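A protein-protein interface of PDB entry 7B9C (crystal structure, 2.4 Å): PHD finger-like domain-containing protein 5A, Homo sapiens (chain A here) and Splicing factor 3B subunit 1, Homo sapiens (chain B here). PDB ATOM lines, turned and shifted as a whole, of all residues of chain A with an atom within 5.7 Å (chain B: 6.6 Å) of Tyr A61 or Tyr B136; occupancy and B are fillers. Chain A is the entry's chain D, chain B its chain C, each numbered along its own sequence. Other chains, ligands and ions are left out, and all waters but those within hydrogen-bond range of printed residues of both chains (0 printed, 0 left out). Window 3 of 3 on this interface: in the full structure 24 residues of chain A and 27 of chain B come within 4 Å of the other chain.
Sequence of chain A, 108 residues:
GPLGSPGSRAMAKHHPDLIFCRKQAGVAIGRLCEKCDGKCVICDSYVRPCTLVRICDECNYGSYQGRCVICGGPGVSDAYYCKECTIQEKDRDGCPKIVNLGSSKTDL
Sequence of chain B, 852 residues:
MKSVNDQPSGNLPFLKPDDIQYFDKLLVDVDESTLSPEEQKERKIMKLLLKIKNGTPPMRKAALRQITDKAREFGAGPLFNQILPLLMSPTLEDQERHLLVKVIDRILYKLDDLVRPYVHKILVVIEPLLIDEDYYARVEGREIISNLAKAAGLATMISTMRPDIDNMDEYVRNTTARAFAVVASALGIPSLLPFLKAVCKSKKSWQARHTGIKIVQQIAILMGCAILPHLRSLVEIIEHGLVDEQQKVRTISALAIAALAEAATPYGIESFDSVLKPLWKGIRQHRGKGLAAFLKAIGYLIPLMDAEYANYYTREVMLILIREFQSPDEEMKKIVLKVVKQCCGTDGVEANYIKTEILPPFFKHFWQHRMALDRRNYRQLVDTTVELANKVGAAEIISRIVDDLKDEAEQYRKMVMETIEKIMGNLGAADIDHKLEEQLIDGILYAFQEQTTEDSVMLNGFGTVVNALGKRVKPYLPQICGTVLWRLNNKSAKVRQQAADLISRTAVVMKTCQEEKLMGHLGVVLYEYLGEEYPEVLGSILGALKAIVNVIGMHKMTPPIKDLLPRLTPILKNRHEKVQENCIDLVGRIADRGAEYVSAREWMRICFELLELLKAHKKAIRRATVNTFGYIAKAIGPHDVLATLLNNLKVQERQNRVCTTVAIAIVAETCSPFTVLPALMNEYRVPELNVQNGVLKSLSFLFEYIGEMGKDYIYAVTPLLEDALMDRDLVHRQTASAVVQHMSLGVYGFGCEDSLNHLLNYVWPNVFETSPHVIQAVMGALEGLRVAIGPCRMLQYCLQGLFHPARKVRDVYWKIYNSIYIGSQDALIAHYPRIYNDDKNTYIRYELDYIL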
ATOM      1  N   ASP A  57     -14.009 -10.342  19.230  1.00  0.00           N
ATOM      2  CA  ASP A  57     -14.650  -9.772  18.052  1.00  0.00           C
ATOM      3  C   ASP A  57     -16.005  -9.169  18.395  1.00  0.00           C
ATOM      4  O   ASP A  57     -16.408  -8.157  17.809  1.00  0.00           O
ATOM      5  CB  ASP A  57     -14.804 -10.829  16.963  1.00  0.00           C
ATOM      6  CG  ASP A  57     -13.617 -10.881  16.032  1.00  0.00           C
ATOM      7  OD1 ASP A  57     -13.218 -11.995  15.663  1.00  0.00           O
ATOM      8  OD2 ASP A  57     -13.088  -9.810  15.667  1.00  0.00           O
ATOM      9  N   GLU A  58     -16.735  -9.791  19.324  1.00  0.00           N
ATOM     10  CA  GLU A  58     -18.016  -9.234  19.743  1.00  0.00           C
ATOM     11  C   GLU A  58     -17.845  -7.847  20.355  1.00  0.00           C
ATOM     12  O   GLU A  58     -18.685  -6.962  20.148  1.00  0.00           O
ATOM     13  CB  GLU A  58     -18.696 -10.182  20.730  1.00  0.00           C
ATOM     14  CG  GLU A  58     -20.062  -9.702  21.181  1.00  0.00           C
ATOM     15  CD  GLU A  58     -20.452 -10.229  22.548  1.00  0.00           C
ATOM     16  OE1 GLU A  58     -19.835  -9.805  23.552  1.00  0.00           O
ATOM     17  OE2 GLU A  58     -21.385 -11.056  22.618  1.00  0.00           O
ATOM     18  N   CYS A  59     -16.755  -7.633  21.098  1.00  0.00           N
ATOM     19  CA  CYS A  59     -16.506  -6.335  21.716  1.00  0.00           C
ATOM     20  C   CYS A  59     -16.087  -5.266  20.716  1.00  0.00           C
ATOM     21  O   CYS A  59     -16.010  -4.091  21.090  1.00  0.00           O
ATOM     22  CB  CYS A  59     -15.439  -6.470  22.804  1.00  0.00           C
ATOM     23  SG  CYS A  59     -16.032  -7.310  24.292  1.00  0.00           S
ATOM     24  N   ASN A  60     -15.831  -5.635  19.462  1.00  0.00           N
ATOM     25  CA  ASN A  60     -15.389  -4.691  18.444  1.00  0.00           C
ATOM     26  C   ASN A  60     -16.367  -4.575  17.280  1.00  0.00           C
ATOM     27  O   ASN A  60     -16.050  -3.916  16.282  1.00  0.00           O
ATOM     28  CB  ASN A  60     -14.005  -5.095  17.929  1.00  0.00           C
ATOM     29  CG  ASN A  60     -13.251  -3.935  17.310  1.00  0.00           C
ATOM     30  OD1 ASN A  60     -12.939  -3.951  16.120  1.00  0.00           O
ATOM     31  ND2 ASN A  60     -12.960  -2.919  18.116  1.00  0.00           N
ATOM     32  N   TYR A  61     -17.547  -5.184  17.376  1.00  0.00           N
ATOM     33  CA  TYR A  61     -18.459  -5.227  16.242  1.00  0.00           C
ATOM     34  C   TYR A  61     -19.254  -3.934  16.108  1.00  0.00           C
ATOM     35  O   TYR A  61     -19.700  -3.352  17.101  1.00  0.00           O
ATOM     36  CB  TYR A  61     -19.429  -6.404  16.367  1.00  0.00           C
ATOM     37  CG  TYR A  61     -20.464  -6.414  15.265  1.00  0.00           C
ATOM     38  CD1 TYR A  61     -20.172  -6.956  14.022  1.00  0.00           C
ATOM     39  CD2 TYR A  61     -21.724  -5.855  15.458  1.00  0.00           C
ATOM     40  CE1 TYR A  61     -21.107  -6.956  13.005  1.00  0.00           C
ATOM     41  CE2 TYR A  61     -22.663  -5.846  14.446  1.00  0.00           C
ATOM     42  CZ  TYR A  61     -22.349  -6.401  13.223  1.00  0.00           C
ATOM     43  OH  TYR A  61     -23.277  -6.400  12.209  1.00  0.00           O
ATOM     44  N   GLY A  62     -19.438  -3.499  14.863  1.00  0.00           N
ATOM     45  CA  GLY A  62     -20.387  -2.433  14.577  1.00  0.00           C
ATOM     46  C   GLY A  62     -19.961  -1.103  15.163  1.00  0.00           C
ATOM     47  O   GLY A  62     -18.825  -0.647  14.982  1.00  0.00           O
ATOM     48  N   SER A  63     -20.890  -0.463  15.875  1.00  0.00           N
ATOM     49  CA  SER A  63     -20.625   0.825  16.502  1.00  0.00           C
ATOM     50  C   SER A  63     -19.667   0.721  17.681  1.00  0.00           C
ATOM     51  O   SER A  63     -19.206   1.758  18.170  1.00  0.00           O
ATOM     52  CB  SER A  63     -21.940   1.464  16.955  1.00  0.00           C
ATOM     53  OG  SER A  63     -22.713   0.556  17.723  1.00  0.00           O
ATOM     54  N   TYR A  64     -19.356  -0.493  18.144  1.00  0.00           N
ATOM     55  CA  TYR A  64     -18.413  -0.683  19.241  1.00  0.00           C
ATOM     56  C   TYR A  64     -16.958  -0.652  18.790  1.00  0.00           C
ATOM     57  O   TYR A  64     -16.065  -0.672  19.643  1.00  0.00           O
ATOM     58  CB  TYR A  64     -18.684  -2.013  19.952  1.00  0.00           C
ATOM     59  CG  TYR A  64     -19.899  -2.006  20.850  1.00  0.00           C
ATOM     60  CD1 TYR A  64     -20.522  -0.815  21.201  1.00  0.00           C
ATOM     61  CD2 TYR A  64     -20.427  -3.192  21.348  1.00  0.00           C
ATOM     62  CE1 TYR A  64     -21.634  -0.805  22.022  1.00  0.00           C
ATOM     63  CE2 TYR A  64     -21.539  -3.192  22.169  1.00  0.00           C
ATOM     64  CZ  TYR A  64     -22.139  -1.995  22.503  1.00  0.00           C
ATOM     65  OH  TYR A  64     -23.248  -1.986  23.319  1.00  0.00           O
ATOM     66  N   GLN A  65     -16.696  -0.605  17.486  1.00  0.00           N
ATOM     67  CA  GLN A  65     -15.325  -0.677  17.000  1.00  0.00           C
ATOM     68  C   GLN A  65     -14.564   0.602  17.325  1.00  0.00           C
ATOM     69  O   GLN A  65     -15.085   1.711  17.177  1.00  0.00           O
ATOM     70  CB  GLN A  65     -15.313  -0.925  15.493  1.00  0.00           C
ATOM     71  CG  GLN A  65     -13.922  -1.129  14.924  1.00  0.00           C
ATOM     72  CD  GLN A  65     -13.705  -0.381  13.627  1.00  0.00           C
ATOM     73  OE1 GLN A  65     -13.845   0.842  13.572  1.00  0.00           O
ATOM     74  NE2 GLN A  65     -13.344  -1.109  12.577  1.00  0.00           N
ATOM     75  N   ASP B  94     -28.541   0.420  16.876  1.00  0.00           N
ATOM     76  CA  ASP B  94     -27.677  -0.449  16.079  1.00  0.00           C
ATOM     77  C   ASP B  94     -27.364  -1.753  16.805  1.00  0.00           C
ATOM     78  O   ASP B  94     -27.491  -2.843  16.232  1.00  0.00           O
ATOM     79  CB  ASP B  94     -26.387   0.291  15.717  1.00  0.00           C
ATOM     80  CG  ASP B  94     -26.633   1.493  14.820  1.00  0.00           C
ATOM     81  OD1 ASP B  94     -27.810   1.777  14.509  1.00  0.00           O
ATOM     82  OD2 ASP B  94     -25.649   2.152  14.424  1.00  0.00           O
ATOM     83  N   GLN B  95     -26.947  -1.663  18.071  1.00  0.00           N
ATOM     84  CA  GLN B  95     -26.591  -2.874  18.802  1.00  0.00           C
ATOM     85  C   GLN B  95     -27.822  -3.704  19.144  1.00  0.00           C
ATOM     86  O   GLN B  95     -27.727  -4.930  19.259  1.00  0.00           O
ATOM     87  CB  GLN B  95     -25.800  -2.522  20.062  1.00  0.00           C
ATOM     88  CG  GLN B  95     -24.342  -2.173  19.786  1.00  0.00           C
ATOM     89  CD  GLN B  95     -23.499  -3.392  19.435  1.00  0.00           C
ATOM     90  OE1 GLN B  95     -22.643  -3.335  18.552  1.00  0.00           O
ATOM     91  NE2 GLN B  95     -23.744  -4.502  20.121  1.00  0.00           N
ATOM     92  N   ARG B  97     -30.276  -3.983  16.971  1.00  0.00           N
ATOM     93  CA  ARG B  97     -30.406  -4.696  15.705  1.00  0.00           C
ATOM     94  C   ARG B  97     -29.441  -5.870  15.638  1.00  0.00           C
ATOM     95  O   ARG B  97     -29.794  -6.947  15.146  1.00  0.00           O
ATOM     96  CB  ARG B  97     -30.172  -3.743  14.532  1.00  0.00           C
ATOM     97  CG  ARG B  97     -30.919  -4.138  13.267  1.00  0.00           C
ATOM     98  CD  ARG B  97     -30.187  -3.697  12.009  1.00  0.00           C
ATOM     99  NE  ARG B  97     -29.685  -2.330  12.102  1.00  0.00           N
ATOM    100  CZ  ARG B  97     -28.397  -2.004  12.052  1.00  0.00           C
ATOM    101  NH1 ARG B  97     -27.481  -2.950  11.911  1.00  0.00           N
ATOM    102  NH2 ARG B  97     -28.024  -0.735  12.142  1.00  0.00           N
ATOM    103  N   HIS B  98     -28.219  -5.684  16.141  1.00  0.00           N
ATOM    104  CA  HIS B  98     -27.257  -6.780  16.160  1.00  0.00           C
ATOM    105  C   HIS B  98     -27.732  -7.916  17.060  1.00  0.00           C
ATOM    106  O   HIS B  98     -27.599  -9.096  16.711  1.00  0.00           O
ATOM    107  CB  HIS B  98     -25.890  -6.264  16.610  1.00  0.00           C
ATOM    108  CG  HIS B  98     -24.847  -7.331  16.724  1.00  0.00           C
ATOM    109  ND1 HIS B  98     -24.454  -8.105  15.653  1.00  0.00           N
ATOM    110  CD2 HIS B  98     -24.117  -7.754  17.783  1.00  0.00           C
ATOM    111  CE1 HIS B  98     -23.523  -8.957  16.047  1.00  0.00           C
ATOM    112  NE2 HIS B  98     -23.302  -8.766  17.335  1.00  0.00           N
ATOM    113  N   VAL B 101     -30.327  -9.776  15.228  1.00  0.00           N
ATOM    114  CA  VAL B 101     -29.733 -10.571  14.157  1.00  0.00           C
ATOM    115  C   VAL B 101     -29.122 -11.850  14.720  1.00  0.00           C
ATOM    116  O   VAL B 101     -29.238 -12.928  14.124  1.00  0.00           O
ATOM    117  CB  VAL B 101     -28.698  -9.731  13.385  1.00  0.00           C
ATOM    118  CG1 VAL B 101     -27.806 -10.623  12.536  1.00  0.00           C
ATOM    119  CG2 VAL B 101     -29.396  -8.699  12.519  1.00  0.00           C
ATOM    120  N   LEU B 129     -32.453  -4.068   4.090  1.00  0.00           N
ATOM    121  CA  LEU B 129     -31.200  -3.904   4.817  1.00  0.00           C
ATOM    122  C   LEU B 129     -29.996  -3.978   3.887  1.00  0.00           C
ATOM    123  O   LEU B 129     -28.953  -3.385   4.182  1.00  0.00           O
ATOM    124  CB  LEU B 129     -31.079  -4.966   5.910  1.00  0.00           C
ATOM    125  CG  LEU B 129     -32.024  -4.859   7.107  1.00  0.00           C
ATOM    126  CD1 LEU B 129     -31.823  -6.042   8.041  1.00  0.00           C
ATOM    127  CD2 LEU B 129     -31.815  -3.548   7.845  1.00  0.00           C
ATOM    128  N   GLU B 133     -27.671   2.531   4.135  1.00  0.00           N
ATOM    129  CA  GLU B 133     -26.436   3.307   4.159  1.00  0.00           C
ATOM    130  C   GLU B 133     -25.446   2.755   5.175  1.00  0.00           C
ATOM    131  O   GLU B 133     -24.231   2.815   4.955  1.00  0.00           O
ATOM    132  CB  GLU B 133     -26.741   4.773   4.465  1.00  0.00           C
ATOM    133  CG  GLU B 133     -27.905   5.346   3.678  1.00  0.00           C
ATOM    134  CD  GLU B 133     -27.627   6.748   3.175  1.00  0.00           C
ATOM    135  OE1 GLU B 133     -27.226   6.890   2.000  1.00  0.00           O
ATOM    136  OE2 GLU B 133     -27.806   7.708   3.955  1.00  0.00           O
ATOM    137  N   ASP B 134     -25.942   2.221   6.290  1.00  0.00           N
ATOM    138  CA  ASP B 134     -25.074   1.645   7.306  1.00  0.00           C
ATOM    139  C   ASP B 134     -24.411   0.384   6.762  1.00  0.00           C
ATOM    140  O   ASP B 134     -25.094  -0.545   6.318  1.00  0.00           O
ATOM    141  CB  ASP B 134     -25.876   1.339   8.570  1.00  0.00           C
ATOM    142  CG  ASP B 134     -24.993   1.037   9.770  1.00  0.00           C
ATOM    143  OD1 ASP B 134     -23.759   0.935   9.602  1.00  0.00           O
ATOM    144  OD2 ASP B 134     -25.538   0.898  10.886  1.00  0.00           O
ATOM    145  N   TYR B 135     -23.076   0.364   6.788  1.00  0.00           N
ATOM    146  CA  TYR B 135     -22.332  -0.802   6.321  1.00  0.00           C
ATOM    147  C   TYR B 135     -22.703  -2.047   7.121  1.00  0.00           C
ATOM    148  O   TYR B 135     -22.917  -3.126   6.550  1.00  0.00           O
ATOM    149  CB  TYR B 135     -20.830  -0.511   6.408  1.00  0.00           C
ATOM    150  CG  TYR B 135     -19.925  -1.720   6.342  1.00  0.00           C
ATOM    151  CD1 TYR B 135     -19.499  -2.228   5.122  1.00  0.00           C
ATOM    152  CD2 TYR B 135     -19.475  -2.340   7.502  1.00  0.00           C
ATOM    153  CE1 TYR B 135     -18.665  -3.330   5.057  1.00  0.00           C
ATOM    154  CE2 TYR B 135     -18.643  -3.441   7.448  1.00  0.00           C
ATOM    155  CZ  TYR B 135     -18.241  -3.932   6.224  1.00  0.00           C
ATOM    156  OH  TYR B 135     -17.409  -5.029   6.173  1.00  0.00           O
ATOM    157  N   TYR B 136     -22.805  -1.910   8.445  1.00  0.00           N
ATOM    158  CA  TYR B 136     -23.144  -3.055   9.282  1.00  0.00           C
ATOM    159  C   TYR B 136     -24.587  -3.497   9.074  1.00  0.00           C
ATOM    160  O   TYR B 136     -24.906  -4.672   9.280  1.00  0.00           O
ATOM    161  CB  TYR B 136     -22.879  -2.725  10.750  1.00  0.00           C
ATOM    162  CG  TYR B 136     -21.420  -2.453  11.037  1.00  0.00           C
ATOM    163  CD1 TYR B 136     -20.506  -3.495  11.137  1.00  0.00           C
ATOM    164  CD2 TYR B 136     -20.952  -1.155  11.192  1.00  0.00           C
ATOM    165  CE1 TYR B 136     -19.168  -3.252  11.393  1.00  0.00           C
ATOM    166  CE2 TYR B 136     -19.619  -0.901  11.447  1.00  0.00           C
ATOM    167  CZ  TYR B 136     -18.730  -1.952  11.547  1.00  0.00           C
ATOM    168  OH  TYR B 136     -17.401  -1.701  11.805  1.00  0.00           O
ATOM    169  N   ALA B 137     -25.464  -2.587   8.643  1.00  0.00           N
ATOM    170  CA  ALA B 137     -26.822  -2.988   8.294  1.00  0.00           C
ATOM    171  C   ALA B 137     -26.825  -3.922   7.090  1.00  0.00           C
ATOM    172  O   ALA B 137     -27.529  -4.939   7.088  1.00  0.00           O
ATOM    173  CB  ALA B 137     -27.684  -1.757   8.023  1.00  0.00           C
ATOM    174  N   ARG B 138     -26.042  -3.595   6.059  1.00  0.00           N
ATOM    175  CA  ARG B 138     -25.921  -4.488   4.910  1.00  0.00           C
ATOM    176  C   ARG B 138     -25.256  -5.799   5.309  1.00  0.00           C
ATOM    177  O   ARG B 138     -25.637  -6.873   4.822  1.00  0.00           O
ATOM    178  CB  ARG B 138     -25.132  -3.805   3.791  1.00  0.00           C
ATOM    179  CG  ARG B 138     -25.794  -2.555   3.228  1.00  0.00           C
ATOM    180  CD  ARG B 138     -25.058  -2.057   1.992  1.00  0.00           C
ATOM    181  NE  ARG B 138     -23.620  -1.949   2.223  1.00  0.00           N
ATOM    182  CZ  ARG B 138     -23.021  -0.864   2.705  1.00  0.00           C
ATOM    183  NH1 ARG B 138     -21.708  -0.856   2.887  1.00  0.00           N
ATOM    184  NH2 ARG B 138     -23.736   0.213   3.007  1.00  0.00           N
ATOM    185  N   VAL B 139     -24.258  -5.730   6.192  1.00  0.00           N
ATOM    186  CA  VAL B 139     -23.623  -6.946   6.691  1.00  0.00           C
ATOM    187  C   VAL B 139     -24.653  -7.846   7.364  1.00  0.00           C
ATOM    188  O   VAL B 139     -24.688  -9.059   7.128  1.00  0.00           O
ATOM    189  CB  VAL B 139     -22.467  -6.590   7.644  1.00  0.00           C
ATOM    190  CG1 VAL B 139     -22.028  -7.810   8.440  1.00  0.00           C
ATOM    191  CG2 VAL B 139     -21.301  -6.007   6.863  1.00  0.00           C
ATOM    192  N   GLU B 140     -25.525  -7.263   8.191  1.00  0.00           N
ATOM    193  CA  GLU B 140     -26.510  -8.063   8.912  1.00  0.00           C
ATOM    194  C   GLU B 140     -27.610  -8.576   7.991  1.00  0.00           C
ATOM    195  O   GLU B 140     -28.126  -9.679   8.200  1.00  0.00           O
ATOM    196  CB  GLU B 140     -27.103  -7.247  10.060  1.00  0.00           C
ATOM    197  CG  GLU B 140     -26.209  -7.196  11.293  1.00  0.00           C
ATOM    198  CD  GLU B 140     -26.388  -5.921  12.094  1.00  0.00           C
ATOM    199  OE1 GLU B 140     -27.435  -5.260  11.939  1.00  0.00           O
ATOM    200  OE2 GLU B 140     -25.478  -5.576  12.877  1.00  0.00           O
ATOM    201  N   GLY B 141     -27.975  -7.804   6.966  1.00  0.00           N
ATOM    202  CA  GLY B 141     -28.903  -8.315   5.969  1.00  0.00           C
ATOM    203  C   GLY B 141     -28.351  -9.525   5.239  1.00  0.00           C
ATOM    204  O   GLY B 141     -29.034 -10.545   5.087  1.00  0.00           O
ATOM    205  N   GLU B 143     -26.089 -11.466   6.385  1.00  0.00           N
ATOM    206  CA  GLU B 143     -26.001 -12.519   7.391  1.00  0.00           C
ATOM    207  C   GLU B 143     -27.327 -13.258   7.524  1.00  0.00           C
ATOM    208  O   GLU B 143     -27.368 -14.496   7.547  1.00  0.00           O
ATOM    209  CB  GLU B 143     -25.584 -11.903   8.726  1.00  0.00           C
ATOM    210  CG  GLU B 143     -25.121 -12.880   9.784  1.00  0.00           C
ATOM    211  CD  GLU B 143     -24.380 -12.181  10.912  1.00  0.00           C
ATOM    212  OE1 GLU B 143     -23.567 -11.276  10.623  1.00  0.00           O
ATOM    213  OE2 GLU B 143     -24.617 -12.527  12.087  1.00  0.00           O
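OE1 of Gln B95 lies close to O of Tyr A61 (3.3 Å).
The side-chain hydroxyl of Tyr A61 sits at hydrogen-bond distance from the side-chain carboxylate of Glu B140 (2.4 Å).
NH1 of Arg B97 is in salt-bridge range of OE2 of Glu B140 (3.4 Å).
The backbone NH of Tyr B136 sits at hydrogen-bond distance from the side-chain carboxylate of Asp B134, 3.2 Å away.
His B98 touches Tyr A61 (ND1 to CE2, 3.1 Å).
Tyr B136 touches Tyr A61.
Gly A62 touches Tyr B136.
OG of Ser A63 touches CG of Gln B95, 3.8 Å away.
Gln B95 touches Tyr A64 (NE2 to CE2, 3.3 Å).
Cys A59 touches none of the printed residues of chain B.
Printed residues of chain B within 4 Å of Ser A63: Gln B95 (3.8 Å).
Printed residues of chain B within 4 Å of Tyr A64: Gln B95.
Asp B94 touches none of the printed residues of chain A.
Printed residues of chain A within 4 Å of Gln B95: Tyr A61 (3.3 Å), Ser A63 (3.8 Å) and Tyr A64 (3.3 Å).
Of the printed residues of chain A, His B98 touches Tyr A61.
Of chain A, only Tyr A61 (3.8 Å) and Gly A62 (3.5 Å) come within 4 Å of Tyr B136.
The nearest residue of chain B that does not touch Tyr A61 is Val B139 (4.2 Å).
The nearest residue of chain A that does not touch Tyr B136 is Gln A65 (4.2 Å).
The nearest printed residue of chain B that does not touch Gly A62 is Gln B95 (4.7 Å).
Of the 16 printed residues of chain B, 4 touch a printed residue of chain A.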
